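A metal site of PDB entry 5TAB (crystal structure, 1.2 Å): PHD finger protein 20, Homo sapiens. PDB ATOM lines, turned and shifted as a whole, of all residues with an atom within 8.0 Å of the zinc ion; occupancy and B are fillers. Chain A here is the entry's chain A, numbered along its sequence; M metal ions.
The backbone carbonyl oxygen (O) of Cys 10 lies close to the side-chain hydroxyl (OH) of Tyr 50 (3.4 Å). SG of Cys 12 lies close to N of Val 14. NE2 of His 32 sits at hydrogen-bond distance from O of Glu 16, at 2.8 Å.
Of the 20 residues printed, 4 come within 4 Å of the zinc ion. The nearest printed residue that does not touch the zinc ion is Ile 11 (4.6 Å).
The zinc ion is bound by a ring nitrogen (ND1) of His 32, the side-chain sulfur (SG) of Cys 12, the side-chain sulfur (SG) of Cys 35 and the side-chain sulfur (SG) of Cys 10.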
ATOM      1  N   VAL A   8     -23.523  18.440 -10.085  1.00  0.00           N
ATOM      2  CA  VAL A   8     -24.474  17.376 -10.409  1.00  0.00           C
ATOM      3  C   VAL A   8     -23.698  16.070 -10.402  1.00  0.00           C
ATOM      4  O   VAL A   8     -22.778  15.873 -11.215  1.00  0.00           O
ATOM      5  CB  VAL A   8     -25.165  17.595 -11.754  1.00  0.00           C
ATOM      6  CG1 VAL A   8     -26.104  16.431 -12.060  1.00  0.00           C
ATOM      7  CG2 VAL A   8     -25.955  18.922 -11.744  1.00  0.00           C
ATOM      8  N   ARG A   9     -23.987  15.209  -9.434  1.00  0.00           N
ATOM      9  CA  ARG A   9     -23.273  13.927  -9.310  1.00  0.00           C
ATOM     10  C   ARG A   9     -24.316  12.858  -9.036  1.00  0.00           C
ATOM     11  O   ARG A   9     -24.690  12.594  -7.889  1.00  0.00           O
ATOM     12  CB  ARG A   9     -22.185  13.976  -8.258  1.00  0.00           C
ATOM     13  CG  ARG A   9     -21.181  12.826  -8.410  1.00  0.00           C
ATOM     14  CD  ARG A   9     -21.556  11.636  -7.570  1.00  0.00           C
ATOM     15  NE  ARG A   9     -21.227  11.766  -6.158  1.00  0.00           N
ATOM     16  CZ  ARG A   9     -22.086  11.773  -5.122  1.00  0.00           C
ATOM     17  NH1 ARG A   9     -23.395  11.799  -5.327  1.00  0.00           N
ATOM     18  NH2 ARG A   9     -21.634  11.774  -3.881  1.00  0.00           N
ATOM     19  N   CYS A  10     -24.815  12.281 -10.120  1.00  0.00           N
ATOM     20  CA  CYS A  10     -25.932  11.352 -10.043  1.00  0.00           C
ATOM     21  C   CYS A  10     -25.492  10.001 -10.574  1.00  0.00           C
ATOM     22  O   CYS A  10     -24.568   9.905 -11.389  1.00  0.00           O
ATOM     23  CB  CYS A  10     -27.122  11.903 -10.845  1.00  0.00           C
ATOM     24  SG  CYS A  10     -28.676  11.019 -10.481  1.00  0.00           S
ATOM     25  N   ILE A  11     -26.221   8.949 -10.202  1.00  0.00           N
ATOM     26  CA  ILE A  11     -25.825   7.583 -10.589  1.00  0.00           C
ATOM     27  C   ILE A  11     -25.946   7.352 -12.088  1.00  0.00           C
ATOM     28  O   ILE A  11     -25.298   6.482 -12.642  1.00  0.00           O
ATOM     29  CB  ILE A  11     -26.699   6.566  -9.770  1.00  0.00           C
ATOM     30  CG1 ILE A  11     -26.154   5.147  -9.914  1.00  0.00           C
ATOM     31  CG2 ILE A  11     -28.182   6.666 -10.200  1.00  0.00           C
ATOM     32  CD1 ILE A  11     -26.890   4.175  -8.986  1.00  0.00           C
ATOM     33  N   CYS A  12     -26.776   8.149 -12.755  1.00  0.00           N
ATOM     34  CA  CYS A  12     -26.923   8.061 -14.202  1.00  0.00           C
ATOM     35  C   CYS A  12     -25.740   8.664 -14.962  1.00  0.00           C
ATOM     36  O   CYS A  12     -25.612   8.437 -16.158  1.00  0.00           O
ATOM     37  CB  CYS A  12     -28.228   8.774 -14.611  1.00  0.00           C
ATOM     38  SG  CYS A  12     -28.125  10.566 -14.320  1.00  0.00           S
ATOM     39  N   GLU A  13     -24.889   9.409 -14.251  1.00  0.00           N
ATOM     40  CA  GLU A  13     -23.701  10.086 -14.801  1.00  0.00           C
ATOM     41  C   GLU A  13     -24.050  11.114 -15.878  1.00  0.00           C
ATOM     42  O   GLU A  13     -23.210  11.452 -16.694  1.00  0.00           O
ATOM     43  CB  GLU A  13     -22.669   9.078 -15.335  1.00  0.00           C
ATOM     44  CG  GLU A  13     -22.124   8.213 -14.181  1.00  0.00           C
ATOM     45  CD  GLU A  13     -20.789   7.586 -14.464  1.00  0.00           C
ATOM     46  OE1 GLU A  13     -19.893   8.319 -14.918  1.00  0.00           O
ATOM     47  OE2 GLU A  13     -20.609   6.391 -14.209  1.00  0.00           O
ATOM     48  N   VAL A  14     -25.265  11.610 -15.862  1.00  0.00           N
ATOM     49  CA  VAL A  14     -25.668  12.715 -16.748  1.00  0.00           C
ATOM     50  C   VAL A  14     -25.564  14.025 -15.946  1.00  0.00           C
ATOM     51  O   VAL A  14     -26.097  14.139 -14.848  1.00  0.00           O
ATOM     52  CB  VAL A  14     -27.097  12.480 -17.303  1.00  0.00           C
ATOM     53  CG1 VAL A  14     -27.569  13.699 -18.101  1.00  0.00           C
ATOM     54  CG2 VAL A  14     -27.102  11.213 -18.162  1.00  0.00           C
ATOM     55  N   GLN A  15     -24.857  15.004 -16.513  1.00  0.00           N
ATOM     56  CA  GLN A  15     -24.637  16.297 -15.860  1.00  0.00           C
ATOM     57  C   GLN A  15     -25.814  17.249 -16.039  1.00  0.00           C
ATOM     58  O   GLN A  15     -26.050  18.135 -15.231  1.00  0.00           O
ATOM     59  CB  GLN A  15     -23.326  16.949 -16.391  1.00  0.00           C
ATOM     60  CG  GLN A  15     -23.037  18.387 -15.859  1.00  0.00           C
ATOM     61  CD  GLN A  15     -21.682  18.918 -16.310  1.00  0.00           C
ATOM     62  OE1 GLN A  15     -20.866  18.171 -16.861  1.00  0.00           O
ATOM     63  NE2 GLN A  15     -21.430  20.212 -16.094  1.00  0.00           N
ATOM     64  N   GLU A  16     -26.528  17.102 -17.131  1.00  0.00           N
ATOM     65  CA  GLU A  16     -27.642  17.988 -17.450  1.00  0.00           C
ATOM     66  C   GLU A  16     -28.758  17.837 -16.427  1.00  0.00           C
ATOM     67  O   GLU A  16     -29.153  16.709 -16.091  1.00  0.00           O
ATOM     68  CB  GLU A  16     -28.207  17.669 -18.841  1.00  0.00           C
ATOM     69  CG  GLU A  16     -27.328  18.150 -19.980  1.00  0.00           C
ATOM     70  CD  GLU A  16     -25.886  17.595 -19.919  1.00  0.00           C
ATOM     71  OE1 GLU A  16     -24.923  18.442 -19.940  1.00  0.00           O
ATOM     72  OE2 GLU A  16     -25.711  16.346 -19.875  1.00  0.00           O
ATOM     73  N   ASN A  18     -32.677  18.271 -14.960  1.00  0.00           N
ATOM     74  CA  ASN A  18     -34.047  18.175 -15.461  1.00  0.00           C
ATOM     75  C   ASN A  18     -34.946  19.062 -14.603  1.00  0.00           C
ATOM     76  O   ASN A  18     -34.493  20.091 -14.120  1.00  0.00           O
ATOM     77  CB  ASN A  18     -34.518  16.713 -15.523  1.00  0.00           C
ATOM     78  CG  ASN A  18     -34.593  16.060 -14.143  1.00  0.00           C
ATOM     79  OD1 ASN A  18     -34.341  16.687 -13.129  1.00  0.00           O
ATOM     80  ND2 ASN A  18     -34.918  14.784 -14.120  1.00  0.00           N
ATOM     81  N   PHE A  20     -36.410  18.248 -11.687  1.00  0.00           N
ATOM     82  CA  PHE A  20     -36.537  17.828 -10.278  1.00  0.00           C
ATOM     83  C   PHE A  20     -35.178  17.354  -9.814  1.00  0.00           C
ATOM     84  O   PHE A  20     -34.871  16.157  -9.882  1.00  0.00           O
ATOM     85  CB  PHE A  20     -37.642  16.780 -10.120  1.00  0.00           C
ATOM     86  CG  PHE A  20     -37.779  16.230  -8.718  1.00  0.00           C
ATOM     87  CD1 PHE A  20     -37.682  17.066  -7.605  1.00  0.00           C
ATOM     88  CD2 PHE A  20     -37.987  14.881  -8.513  1.00  0.00           C
ATOM     89  CE1 PHE A  20     -37.800  16.563  -6.306  1.00  0.00           C
ATOM     90  CE2 PHE A  20     -38.101  14.389  -7.173  1.00  0.00           C
ATOM     91  CZ  PHE A  20     -37.979  15.243  -6.112  1.00  0.00           C
ATOM     92  N   MET A  21     -34.399  18.308  -9.300  1.00  0.00           N
ATOM     93  CA  MET A  21     -33.062  18.067  -8.754  1.00  0.00           C
ATOM     94  C   MET A  21     -33.140  18.167  -7.225  1.00  0.00           C
ATOM     95  O   MET A  21     -33.862  19.030  -6.697  1.00  0.00           O
ATOM     96  CB  MET A  21     -32.095  19.145  -9.266  1.00  0.00           C
ATOM     97  CG  MET A  21     -32.068  19.248 -10.787  1.00  0.00           C
ATOM     98  SD  MET A  21     -31.555  17.698 -11.589  1.00  0.00           S
ATOM     99  CE  MET A  21     -29.822  17.597 -11.145  1.00  0.00           C
ATOM    100  N   TRP A  30     -25.841  17.294  -6.102  1.00  0.00           N
ATOM    101  CA  TRP A  30     -27.229  17.179  -6.533  1.00  0.00           C
ATOM    102  C   TRP A  30     -27.430  15.952  -7.406  1.00  0.00           C
ATOM    103  O   TRP A  30     -26.565  15.588  -8.199  1.00  0.00           O
ATOM    104  CB  TRP A  30     -27.658  18.427  -7.304  1.00  0.00           C
ATOM    105  CG  TRP A  30     -27.670  19.703  -6.492  1.00  0.00           C
ATOM    106  CD1 TRP A  30     -26.580  20.412  -6.059  1.00  0.00           C
ATOM    107  CD2 TRP A  30     -28.821  20.443  -6.074  1.00  0.00           C
ATOM    108  NE1 TRP A  30     -26.982  21.543  -5.392  1.00  0.00           N
ATOM    109  CE2 TRP A  30     -28.364  21.586  -5.390  1.00  0.00           C
ATOM    110  CE3 TRP A  30     -30.205  20.254  -6.220  1.00  0.00           C
ATOM    111  CZ2 TRP A  30     -29.231  22.536  -4.863  1.00  0.00           C
ATOM    112  CZ3 TRP A  30     -31.069  21.193  -5.683  1.00  0.00           C
ATOM    113  CH2 TRP A  30     -30.581  22.344  -5.031  1.00  0.00           C
ATOM    114  N   GLN A  31     -28.613  15.367  -7.295  1.00  0.00           N
ATOM    115  CA  GLN A  31     -29.025  14.220  -8.090  1.00  0.00           C
ATOM    116  C   GLN A  31     -30.369  14.520  -8.751  1.00  0.00           C
ATOM    117  O   GLN A  31     -31.139  15.404  -8.302  1.00  0.00           O
ATOM    118  CB  GLN A  31     -29.182  12.981  -7.202  1.00  0.00           C
ATOM    119  CG  GLN A  31     -27.882  12.523  -6.579  1.00  0.00           C
ATOM    120  CD  GLN A  31     -27.419  13.393  -5.429  1.00  0.00           C
ATOM    121  OE1 GLN A  31     -28.181  13.694  -4.492  1.00  0.00           O
ATOM    122  NE2 GLN A  31     -26.130  13.824  -5.462  1.00  0.00           N
ATOM    123  N   HIS A  32     -30.691  13.766  -9.793  1.00  0.00           N
ATOM    124  CA  HIS A  32     -32.068  13.800 -10.303  1.00  0.00           C
ATOM    125  C   HIS A  32     -32.932  12.984  -9.371  1.00  0.00           C
ATOM    126  O   HIS A  32     -32.647  11.795  -9.091  1.00  0.00           O
ATOM    127  CB  HIS A  32     -32.147  13.188 -11.721  1.00  0.00           C
ATOM    128  CG  HIS A  32     -31.118  13.725 -12.660  1.00  0.00           C
ATOM    129  ND1 HIS A  32     -29.985  13.006 -13.018  1.00  0.00           N
ATOM    130  CD2 HIS A  32     -31.048  14.922 -13.314  1.00  0.00           C
ATOM    131  CE1 HIS A  32     -29.251  13.750 -13.829  1.00  0.00           C
ATOM    132  NE2 HIS A  32     -29.874  14.916 -14.039  1.00  0.00           N
ATOM    133  N   GLY A  33     -34.026  13.573  -8.889  1.00  0.00           N
ATOM    134  CA  GLY A  33     -34.907  12.847  -8.014  1.00  0.00           C
ATOM    135  C   GLY A  33     -35.404  11.529  -8.577  1.00  0.00           C
ATOM    136  O   GLY A  33     -35.491  10.524  -7.853  1.00  0.00           O
ATOM    137  N   VAL A  34     -35.725  11.501  -9.865  1.00  0.00           N
ATOM    138  CA  VAL A  34     -36.221  10.281 -10.471  1.00  0.00           C
ATOM    139  C   VAL A  34     -35.163   9.153 -10.418  1.00  0.00           C
ATOM    140  O   VAL A  34     -35.470   7.989 -10.189  1.00  0.00           O
ATOM    141  CB  VAL A  34     -36.745  10.540 -11.919  1.00  0.00           C
ATOM    142  CG1 VAL A  34     -35.631  11.013 -12.878  1.00  0.00           C
ATOM    143  CG2 VAL A  34     -37.459   9.302 -12.446  1.00  0.00           C
ATOM    144  N   CYS A  35     -33.898   9.493 -10.592  1.00  0.00           N
ATOM    145  CA  CYS A  35     -32.839   8.485 -10.465  1.00  0.00           C
ATOM    146  C   CYS A  35     -32.760   7.946  -9.057  1.00  0.00           C
ATOM    147  O   CYS A  35     -32.397   6.781  -8.858  1.00  0.00           O
ATOM    148  CB  CYS A  35     -31.490   9.078 -10.882  1.00  0.00           C
ATOM    149  SG  CYS A  35     -31.467   9.627 -12.625  1.00  0.00           S
ATOM    150  N   MET A  36     -33.094   8.789  -8.074  1.00  0.00           N
ATOM    151  CA  MET A  36     -33.036   8.401  -6.658  1.00  0.00           C
ATOM    152  C   MET A  36     -34.325   7.726  -6.210  1.00  0.00           C
ATOM    153  O   MET A  36     -34.478   7.433  -5.037  1.00  0.00           O
ATOM    154  CB  MET A  36     -32.714   9.613  -5.798  1.00  0.00           C
ATOM    155  CG  MET A  36     -31.382  10.266  -6.155  1.00  0.00           C
ATOM    156  SD  MET A  36     -29.939   9.235  -5.849  1.00  0.00           S
ATOM    157  CE  MET A  36     -29.573   8.589  -7.503  1.00  0.00           C
ATOM    158  N   TYR A  50     -27.485   8.250  -3.091  1.00  0.00           N
ATOM    159  CA  TYR A  50     -27.134   6.849  -3.302  1.00  0.00           C
ATOM    160  C   TYR A  50     -25.743   6.514  -2.797  1.00  0.00           C
ATOM    161  O   TYR A  50     -25.489   5.378  -2.378  1.00  0.00           O
ATOM    162  CB  TYR A  50     -27.234   6.497  -4.787  1.00  0.00           C
ATOM    163  CG  TYR A  50     -26.186   7.154  -5.690  1.00  0.00           C
ATOM    164  CD1 TYR A  50     -26.276   8.504  -6.042  1.00  0.00           C
ATOM    165  CD2 TYR A  50     -25.178   6.408  -6.269  1.00  0.00           C
ATOM    166  CE1 TYR A  50     -25.363   9.098  -6.896  1.00  0.00           C
ATOM    167  CE2 TYR A  50     -24.254   6.971  -7.148  1.00  0.00           C
ATOM    168  CZ  TYR A  50     -24.345   8.331  -7.446  1.00  0.00           C
ATOM    169  OH  TYR A  50     -23.445   8.926  -8.306  1.00  0.00           O
HETATM  170 ZN    ZN M   1     -29.609  10.994 -12.632  1.00  0.00          ZN
